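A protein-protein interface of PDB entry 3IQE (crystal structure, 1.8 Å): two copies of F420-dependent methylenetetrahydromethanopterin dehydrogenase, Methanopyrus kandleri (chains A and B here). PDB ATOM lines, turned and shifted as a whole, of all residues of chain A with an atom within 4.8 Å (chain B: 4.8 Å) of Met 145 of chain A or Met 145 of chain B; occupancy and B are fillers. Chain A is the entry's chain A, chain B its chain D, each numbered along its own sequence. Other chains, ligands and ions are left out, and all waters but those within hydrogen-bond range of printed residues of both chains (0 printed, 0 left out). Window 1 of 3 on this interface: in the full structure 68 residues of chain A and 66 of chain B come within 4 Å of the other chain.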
ATOM      1  N   MET A  18      -1.919 -17.958  31.360  1.00  0.00           N
ATOM      2  CA  MET A  18      -0.847 -17.892  30.400  1.00  0.00           C
ATOM      3  C   MET A  18      -1.336 -18.306  29.003  1.00  0.00           C
ATOM      4  O   MET A  18      -0.969 -17.694  28.021  1.00  0.00           O
ATOM      5  CB  MET A  18       0.254 -18.850  30.838  1.00  0.00           C
ATOM      6  CG  MET A  18       1.629 -18.232  30.922  1.00  0.00           C
ATOM      7  SD  MET A  18       2.907 -19.451  31.249  1.00  0.00           S
ATOM      8  CE  MET A  18       4.202 -18.674  30.295  1.00  0.00           C
ATOM      9  N   MET A  19      -2.186 -19.326  28.932  1.00  0.00           N
ATOM     10  CA  MET A  19      -2.595 -19.907  27.671  1.00  0.00           C
ATOM     11  C   MET A  19      -4.033 -19.611  27.214  1.00  0.00           C
ATOM     12  O   MET A  19      -4.397 -19.913  26.063  1.00  0.00           O
ATOM     13  CB  MET A  19      -2.418 -21.437  27.786  1.00  0.00           C
ATOM     14  CG  MET A  19      -1.042 -21.919  27.366  1.00  0.00           C
ATOM     15  SD  MET A  19      -1.054 -22.185  25.584  1.00  0.00           S
ATOM     16  CE  MET A  19       0.703 -22.326  25.257  1.00  0.00           C
ATOM     17  N   ALA A 138      10.447 -21.177  34.944  1.00  0.00           N
ATOM     18  CA  ALA A 138       9.956 -21.575  33.617  1.00  0.00           C
ATOM     19  C   ALA A 138       9.810 -23.092  33.499  1.00  0.00           C
ATOM     20  O   ALA A 138       8.869 -23.613  32.873  1.00  0.00           O
ATOM     21  CB  ALA A 138      10.840 -20.988  32.516  1.00  0.00           C
ATOM     22  N   ASN A 141       6.583 -24.005  35.104  1.00  0.00           N
ATOM     23  CA  ASN A 141       5.467 -23.717  34.258  1.00  0.00           C
ATOM     24  C   ASN A 141       5.369 -24.689  33.127  1.00  0.00           C
ATOM     25  O   ASN A 141       4.280 -24.986  32.655  1.00  0.00           O
ATOM     26  CB  ASN A 141       5.597 -22.288  33.726  1.00  0.00           C
ATOM     27  CG  ASN A 141       4.972 -21.299  34.645  1.00  0.00           C
ATOM     28  OD1 ASN A 141       3.765 -21.117  34.621  1.00  0.00           O
ATOM     29  ND2 ASN A 141       5.777 -20.668  35.483  1.00  0.00           N
ATOM     30  N   ALA A 142       6.515 -25.168  32.673  1.00  0.00           N
ATOM     31  CA  ALA A 142       6.554 -26.168  31.604  1.00  0.00           C
ATOM     32  C   ALA A 142       5.838 -27.449  32.010  1.00  0.00           C
ATOM     33  O   ALA A 142       5.000 -28.010  31.244  1.00  0.00           O
ATOM     34  CB  ALA A 142       8.005 -26.423  31.199  1.00  0.00           C
ATOM     35  N   ASP A 143       6.181 -27.918  33.205  1.00  0.00           N
ATOM     36  CA  ASP A 143       5.599 -29.118  33.745  1.00  0.00           C
ATOM     37  C   ASP A 143       4.128 -28.937  33.979  1.00  0.00           C
ATOM     38  O   ASP A 143       3.320 -29.770  33.569  1.00  0.00           O
ATOM     39  CB  ASP A 143       6.337 -29.517  35.024  1.00  0.00           C
ATOM     40  CG  ASP A 143       7.667 -30.204  34.740  1.00  0.00           C
ATOM     41  OD1 ASP A 143       7.765 -30.868  33.673  1.00  0.00           O
ATOM     42  OD2 ASP A 143       8.629 -30.106  35.552  1.00  0.00           O
ATOM     43  N   LEU A 144       3.771 -27.830  34.609  1.00  0.00           N
ATOM     44  CA  LEU A 144       2.369 -27.497  34.846  1.00  0.00           C
ATOM     45  C   LEU A 144       1.562 -27.401  33.533  1.00  0.00           C
ATOM     46  O   LEU A 144       0.436 -27.920  33.460  1.00  0.00           O
ATOM     47  CB  LEU A 144       2.255 -26.192  35.652  1.00  0.00           C
ATOM     48  CG  LEU A 144       0.828 -25.738  35.957  1.00  0.00           C
ATOM     49  CD1 LEU A 144      -0.048 -26.792  36.660  1.00  0.00           C
ATOM     50  CD2 LEU A 144       0.889 -24.440  36.782  1.00  0.00           C
ATOM     51  N   MET A 145       2.091 -26.711  32.514  1.00  0.00           N
ATOM     52  CA  MET A 145       1.408 -26.652  31.222  1.00  0.00           C
ATOM     53  C   MET A 145       1.156 -28.053  30.666  1.00  0.00           C
ATOM     54  O   MET A 145       0.092 -28.341  30.116  1.00  0.00           O
ATOM     55  CB  MET A 145       2.200 -25.809  30.206  1.00  0.00           C
ATOM     56  CG  MET A 145       1.469 -25.550  28.896  1.00  0.00           C
ATOM     57  SD  MET A 145       2.481 -24.517  27.845  1.00  0.00           S
ATOM     58  CE  MET A 145       2.719 -23.081  28.803  1.00  0.00           C
ATOM     59  N   LYS A 146       2.139 -28.921  30.794  1.00  0.00           N
ATOM     60  CA  LYS A 146       1.989 -30.309  30.338  1.00  0.00           C
ATOM     61  C   LYS A 146       0.815 -31.013  31.041  1.00  0.00           C
ATOM     62  O   LYS A 146      -0.050 -31.662  30.402  1.00  0.00           O
ATOM     63  CB  LYS A 146       3.297 -31.076  30.551  1.00  0.00           C
ATOM     64  CG  LYS A 146       3.323 -32.493  29.988  1.00  0.00           C
ATOM     65  CD  LYS A 146       2.839 -32.508  28.580  1.00  0.00           C
ATOM     66  CE  LYS A 146       2.867 -33.908  27.983  1.00  0.00           C
ATOM     67  NZ  LYS A 146       4.255 -34.488  27.881  1.00  0.00           N
ATOM     68  N   VAL A 147       0.791 -30.905  32.362  1.00  0.00           N
ATOM     69  CA  VAL A 147      -0.327 -31.413  33.162  1.00  0.00           C
ATOM     70  C   VAL A 147      -1.696 -30.827  32.714  1.00  0.00           C
ATOM     71  O   VAL A 147      -2.615 -31.581  32.403  1.00  0.00           O
ATOM     72  CB  VAL A 147      -0.096 -31.140  34.682  1.00  0.00           C
ATOM     73  CG1 VAL A 147      -1.343 -31.468  35.439  1.00  0.00           C
ATOM     74  CG2 VAL A 147       1.109 -31.961  35.202  1.00  0.00           C
ATOM     75  N   LEU A 148      -1.849 -29.499  32.644  1.00  0.00           N
ATOM     76  CA  LEU A 148      -3.154 -28.943  32.346  1.00  0.00           C
ATOM     77  C   LEU A 148      -3.595 -29.245  30.893  1.00  0.00           C
ATOM     78  O   LEU A 148      -4.790 -29.392  30.617  1.00  0.00           O
ATOM     79  CB  LEU A 148      -3.161 -27.429  32.548  1.00  0.00           C
ATOM     80  CG  LEU A 148      -2.913 -27.032  33.988  1.00  0.00           C
ATOM     81  CD1 LEU A 148      -2.737 -25.548  34.145  1.00  0.00           C
ATOM     82  CD2 LEU A 148      -4.095 -27.546  34.798  1.00  0.00           C
ATOM     83  N   ALA A 149      -2.630 -29.356  29.984  1.00  0.00           N
ATOM     84  CA  ALA A 149      -2.918 -29.724  28.602  1.00  0.00           C
ATOM     85  C   ALA A 149      -3.243 -31.196  28.380  1.00  0.00           C
ATOM     86  O   ALA A 149      -4.338 -31.518  27.957  1.00  0.00           O
ATOM     87  CB  ALA A 149      -1.776 -29.285  27.704  1.00  0.00           C
ATOM     88  N   ALA A 150      -2.320 -32.089  28.767  1.00  0.00           N
ATOM     89  CA  ALA A 150      -2.428 -33.513  28.484  1.00  0.00           C
ATOM     90  C   ALA A 150      -3.582 -34.187  29.256  1.00  0.00           C
ATOM     91  O   ALA A 150      -4.200 -35.121  28.755  1.00  0.00           O
ATOM     92  CB  ALA A 150      -1.070 -34.204  28.766  1.00  0.00           C
ATOM     93  N   PHE A 154      -7.257 -28.108  29.774  1.00  0.00           N
ATOM     94  CA  PHE A 154      -7.322 -26.953  28.869  1.00  0.00           C
ATOM     95  C   PHE A 154      -8.505 -27.085  27.935  1.00  0.00           C
ATOM     96  O   PHE A 154      -9.055 -26.102  27.528  1.00  0.00           O
ATOM     97  CB  PHE A 154      -6.043 -26.755  28.051  1.00  0.00           C
ATOM     98  CG  PHE A 154      -4.952 -26.038  28.783  1.00  0.00           C
ATOM     99  CD1 PHE A 154      -3.632 -26.150  28.379  1.00  0.00           C
ATOM    100  CD2 PHE A 154      -5.238 -25.290  29.911  1.00  0.00           C
ATOM    101  CE1 PHE A 154      -2.610 -25.517  29.096  1.00  0.00           C
ATOM    102  CE2 PHE A 154      -4.222 -24.674  30.633  1.00  0.00           C
ATOM    103  CZ  PHE A 154      -2.918 -24.765  30.211  1.00  0.00           C
ATOM    104  N   MET B  18       6.578 -15.586  25.162  1.00  0.00           N
ATOM    105  CA  MET B  18       5.590 -15.955  26.164  1.00  0.00           C
ATOM    106  C   MET B  18       6.149 -15.780  27.591  1.00  0.00           C
ATOM    107  O   MET B  18       5.410 -15.490  28.514  1.00  0.00           O
ATOM    108  CB  MET B  18       5.125 -17.397  25.864  1.00  0.00           C
ATOM    109  CG  MET B  18       4.458 -18.179  26.985  1.00  0.00           C
ATOM    110  SD  MET B  18       3.644 -19.684  26.271  1.00  0.00           S
ATOM    111  CE  MET B  18       2.154 -18.880  25.723  1.00  0.00           C
ATOM    112  N   MET B  19       7.458 -15.923  27.764  1.00  0.00           N
ATOM    113  CA  MET B  19       8.046 -15.927  29.093  1.00  0.00           C
ATOM    114  C   MET B  19       8.892 -14.697  29.331  1.00  0.00           C
ATOM    115  O   MET B  19       9.337 -14.467  30.453  1.00  0.00           O
ATOM    116  CB  MET B  19       8.925 -17.161  29.291  1.00  0.00           C
ATOM    117  CG  MET B  19       8.186 -18.411  29.849  1.00  0.00           C
ATOM    118  SD  MET B  19       7.906 -18.335  31.644  1.00  0.00           S
ATOM    119  CE  MET B  19       9.500 -17.817  32.244  1.00  0.00           C
ATOM    120  N   ALA B 138      -0.659 -26.498  23.114  1.00  0.00           N
ATOM    121  CA  ALA B 138      -0.169 -26.361  24.498  1.00  0.00           C
ATOM    122  C   ALA B 138       0.902 -27.389  24.879  1.00  0.00           C
ATOM    123  O   ALA B 138       1.863 -27.039  25.530  1.00  0.00           O
ATOM    124  CB  ALA B 138      -1.333 -26.448  25.458  1.00  0.00           C
ATOM    125  N   ASN B 141       4.008 -26.249  23.322  1.00  0.00           N
ATOM    126  CA  ASN B 141       4.604 -25.195  24.104  1.00  0.00           C
ATOM    127  C   ASN B 141       5.266 -25.663  25.416  1.00  0.00           C
ATOM    128  O   ASN B 141       6.294 -25.104  25.781  1.00  0.00           O
ATOM    129  CB  ASN B 141       3.622 -24.048  24.327  1.00  0.00           C
ATOM    130  CG  ASN B 141       3.694 -23.050  23.201  1.00  0.00           C
ATOM    131  OD1 ASN B 141       4.559 -22.184  23.193  1.00  0.00           O
ATOM    132  ND2 ASN B 141       2.808 -23.186  22.229  1.00  0.00           N
ATOM    133  N   ALA B 142       4.724 -26.686  26.091  1.00  0.00           N
ATOM    134  CA  ALA B 142       5.279 -27.157  27.379  1.00  0.00           C
ATOM    135  C   ALA B 142       6.663 -27.728  27.112  1.00  0.00           C
ATOM    136  O   ALA B 142       7.613 -27.469  27.845  1.00  0.00           O
ATOM    137  CB  ALA B 142       4.384 -28.241  28.001  1.00  0.00           C
ATOM    138  N   ASP B 143       6.761 -28.509  26.044  1.00  0.00           N
ATOM    139  CA  ASP B 143       8.015 -29.191  25.720  1.00  0.00           C
ATOM    140  C   ASP B 143       9.060 -28.156  25.329  1.00  0.00           C
ATOM    141  O   ASP B 143      10.183 -28.158  25.779  1.00  0.00           O
ATOM    142  CB  ASP B 143       7.763 -30.162  24.597  1.00  0.00           C
ATOM    143  CG  ASP B 143       7.134 -31.460  25.074  1.00  0.00           C
ATOM    144  OD1 ASP B 143       7.294 -31.810  26.264  1.00  0.00           O
ATOM    145  OD2 ASP B 143       6.516 -32.172  24.243  1.00  0.00           O
ATOM    146  N   LEU B 144       8.683 -27.272  24.436  1.00  0.00           N
ATOM    147  CA  LEU B 144       9.560 -26.165  24.057  1.00  0.00           C
ATOM    148  C   LEU B 144      10.010 -25.286  25.230  1.00  0.00           C
ATOM    149  O   LEU B 144      11.190 -24.924  25.340  1.00  0.00           O
ATOM    150  CB  LEU B 144       8.843 -25.315  23.003  1.00  0.00           C
ATOM    151  CG  LEU B 144       9.626 -24.049  22.646  1.00  0.00           C
ATOM    152  CD1 LEU B 144      10.964 -24.414  21.995  1.00  0.00           C
ATOM    153  CD2 LEU B 144       8.779 -23.094  21.727  1.00  0.00           C
ATOM    154  N   MET B 145       9.101 -24.935  26.138  1.00  0.00           N
ATOM    155  CA  MET B 145       9.475 -24.159  27.337  1.00  0.00           C
ATOM    156  C   MET B 145      10.534 -24.882  28.181  1.00  0.00           C
ATOM    157  O   MET B 145      11.491 -24.264  28.675  1.00  0.00           O
ATOM    158  CB  MET B 145       8.227 -23.886  28.194  1.00  0.00           C
ATOM    159  CG  MET B 145       8.411 -22.798  29.257  1.00  0.00           C
ATOM    160  SD  MET B 145       6.898 -22.510  30.185  1.00  0.00           S
ATOM    161  CE  MET B 145       6.012 -21.573  28.951  1.00  0.00           C
ATOM    162  N   LYS B 146      10.344 -26.182  28.354  1.00  0.00           N
ATOM    163  CA  LYS B 146      11.303 -27.005  29.072  1.00  0.00           C
ATOM    164  C   LYS B 146      12.659 -26.926  28.379  1.00  0.00           C
ATOM    165  O   LYS B 146      13.725 -26.870  29.013  1.00  0.00           O
ATOM    166  CB  LYS B 146      10.829 -28.472  29.077  1.00  0.00           C
ATOM    167  CG  LYS B 146      11.660 -29.462  29.934  1.00  0.00           C
ATOM    168  CD  LYS B 146      11.900 -28.902  31.288  1.00  0.00           C
ATOM    169  CE  LYS B 146      12.614 -29.881  32.180  1.00  0.00           C
ATOM    170  NZ  LYS B 146      11.741 -31.047  32.488  1.00  0.00           N
ATOM    171  N   VAL B 147      12.646 -27.043  27.058  1.00  0.00           N
ATOM    172  CA  VAL B 147      13.900 -26.989  26.337  1.00  0.00           C
ATOM    173  C   VAL B 147      14.605 -25.637  26.492  1.00  0.00           C
ATOM    174  O   VAL B 147      15.765 -25.587  26.861  1.00  0.00           O
ATOM    175  CB  VAL B 147      13.697 -27.319  24.863  1.00  0.00           C
ATOM    176  CG1 VAL B 147      14.938 -26.917  24.082  1.00  0.00           C
ATOM    177  CG2 VAL B 147      13.381 -28.808  24.748  1.00  0.00           C
ATOM    178  N   LEU B 148      13.899 -24.533  26.253  1.00  0.00           N
ATOM    179  CA  LEU B 148      14.525 -23.232  26.404  1.00  0.00           C
ATOM    180  C   LEU B 148      14.992 -22.885  27.817  1.00  0.00           C
ATOM    181  O   LEU B 148      15.930 -22.073  28.006  1.00  0.00           O
ATOM    182  CB  LEU B 148      13.556 -22.165  25.930  1.00  0.00           C
ATOM    183  CG  LEU B 148      13.271 -22.394  24.434  1.00  0.00           C
ATOM    184  CD1 LEU B 148      12.153 -21.494  24.019  1.00  0.00           C
ATOM    185  CD2 LEU B 148      14.523 -22.137  23.628  1.00  0.00           C
ATOM    186  N   ALA B 149      14.290 -23.423  28.808  1.00  0.00           N
ATOM    187  CA  ALA B 149      14.575 -23.145  30.202  1.00  0.00           C
ATOM    188  C   ALA B 149      15.727 -24.038  30.695  1.00  0.00           C
ATOM    189  O   ALA B 149      16.717 -23.551  31.207  1.00  0.00           O
ATOM    190  CB  ALA B 149      13.311 -23.408  31.043  1.00  0.00           C
ATOM    191  N   ALA B 150      15.629 -25.343  30.468  1.00  0.00           N
ATOM    192  CA  ALA B 150      16.589 -26.247  31.070  1.00  0.00           C
ATOM    193  C   ALA B 150      17.947 -26.270  30.371  1.00  0.00           C
ATOM    194  O   ALA B 150      18.953 -26.659  30.976  1.00  0.00           O
ATOM    195  CB  ALA B 150      16.027 -27.624  31.149  1.00  0.00           C
ATOM    196  N   PHE B 154      16.847 -19.298  28.340  1.00  0.00           N
ATOM    197  CA  PHE B 154      16.104 -18.224  29.023  1.00  0.00           C
ATOM    198  C   PHE B 154      17.065 -17.427  29.865  1.00  0.00           C
ATOM    199  O   PHE B 154      16.872 -16.230  30.133  1.00  0.00           O
ATOM    200  CB  PHE B 154      14.982 -18.818  29.872  1.00  0.00           C
ATOM    201  CG  PHE B 154      13.757 -19.191  29.062  1.00  0.00           C
ATOM    202  CD1 PHE B 154      12.820 -20.093  29.543  1.00  0.00           C
ATOM    203  CD2 PHE B 154      13.572 -18.647  27.800  1.00  0.00           C
ATOM    204  CE1 PHE B 154      11.685 -20.399  28.793  1.00  0.00           C
ATOM    205  CE2 PHE B 154      12.443 -18.943  27.029  1.00  0.00           C
ATOM    206  CZ  PHE B 154      11.489 -19.791  27.522  1.00  0.00           C
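The backbone NH of Ala 142 of chain A is in hydrogen-bond range of the side-chain sulfur of Met 145 of chain B.
N of Ala 142 of chain B sits at hydrogen-bond distance from SD of Met 145 of chain A, at 3.6 Å.
The backbone carbonyl oxygen of Ala 138 of chain A lies close to the side-chain sulfur of Met 145 of chain B.
SD of Met 145 of chain A lies close to O of Ala 138 of chain B (3.5 Å).
N of Phe 154 of chain A sits at hydrogen-bond distance from O of Leu 148 of chain A (2.9 Å).
O of Leu 148 of chain B sits at hydrogen-bond distance from N of Phe 154 of chain B, at 2.9 Å.
Met 18 of chain B touches Met 18 of chain A.
Met 19 of chain B touches Met 18 of chain A (SD to CE, 3.96 Å).
Met 18 of chain B touches Met 19 of chain A (CE to CE, 3.8 Å).
Ala 138 of chain A touches Met 19 of chain B (CB to CE, 3.5 Å).
Asn 141 of chain A touches Met 145 of chain B.
Ala 142 of chain A touches Lys 146 of chain B (CB to N, 3.7 Å).
CB of Asn 141 of chain B touches SD of Met 145 of chain A, 3.7 Å away.
CE of Met 145 of chain A touches CE of Met 145 of chain B, 3.6 Å away.
CB of Ala 142 of chain B touches N of Lys 146 of chain A, at 3.6 Å.
Phe 154 of chain A touches Ala 138 of chain B (CD1 to CB, 3.7 Å).
Printed residues of chain B within 4 Å of Met 145 of chain A: Ala 138, Asn 141, Ala 142 and Met 145.
Of chain A, only Met 18, Ala 138, Asn 141, Ala 142 and Met 145 come within 4 Å of Met 145 of chain B.
Of the printed residues of chain B, Ala 149 of chain A touches Ala 138 (3.6 Å).
Printed residues of chain A within 4 Å of Met 19 of chain B: Met 18 and Ala 138.
Of the printed residues of chain B, Met 19 of chain A touches Met 18 and Asn 141.
Printed residues of chain B within 4 Å of Phe 154 of chain A: Ala 138.
Of the printed residues of chain A, Phe 154 of chain B touches Ala 138.
Leu 148 of chain B touches none of the printed residues of chain A.
Ala 150 of chain B touches none of the printed residues of chain A.
The nearest printed residue of chain A that does not touch Met 145 of chain B is Asp 143 of chain A (6.2 Å).
The nearest printed residue of chain B that does not touch Met 19 of chain A is Ala 138 of chain B (4.2 Å).
Of the 14 printed residues of chain A, 9 touch a printed residue of chain B.
Hydrophobic or aromatic side chains of chain A within 4 Å of the printed part of chain B: Met 18, Met 19, Ala 138, Ala 142, Met 145, Ala 149 and Phe 154.
Of the 14 printed residues of chain B, 9 touch a printed residue of chain A.
Hydrophobic or aromatic side chains of chain B within 4 Å of the printed part of chain A: Met 18, Met 19, Ala 138, Ala 142, Met 145, Ala 149 and Phe 154.
Among the printed residues, 20 pairs touch across the chains.
Among the printed residues, no Asp or Glu carboxylate lies within 4 Å of a Lys or Arg side-chain nitrogen of the other chain.
Ala 138 of chain A touches Met 145 of chain B, and with the chains exchanged Met 145 of chain A touches Ala 138 of chain B.
Asn 141 of chain A touches Met 145 of chain B, and with the chains exchanged Met 145 of chain A touches Asn 141 of chain B.
Ala 142 of chain A touches its own counterpart, Ala 142 of chain B.
Ala 142 of chain A touches Met 145 of chain B, and with the chains exchanged Met 145 of chain A touches Ala 142 of chain B.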
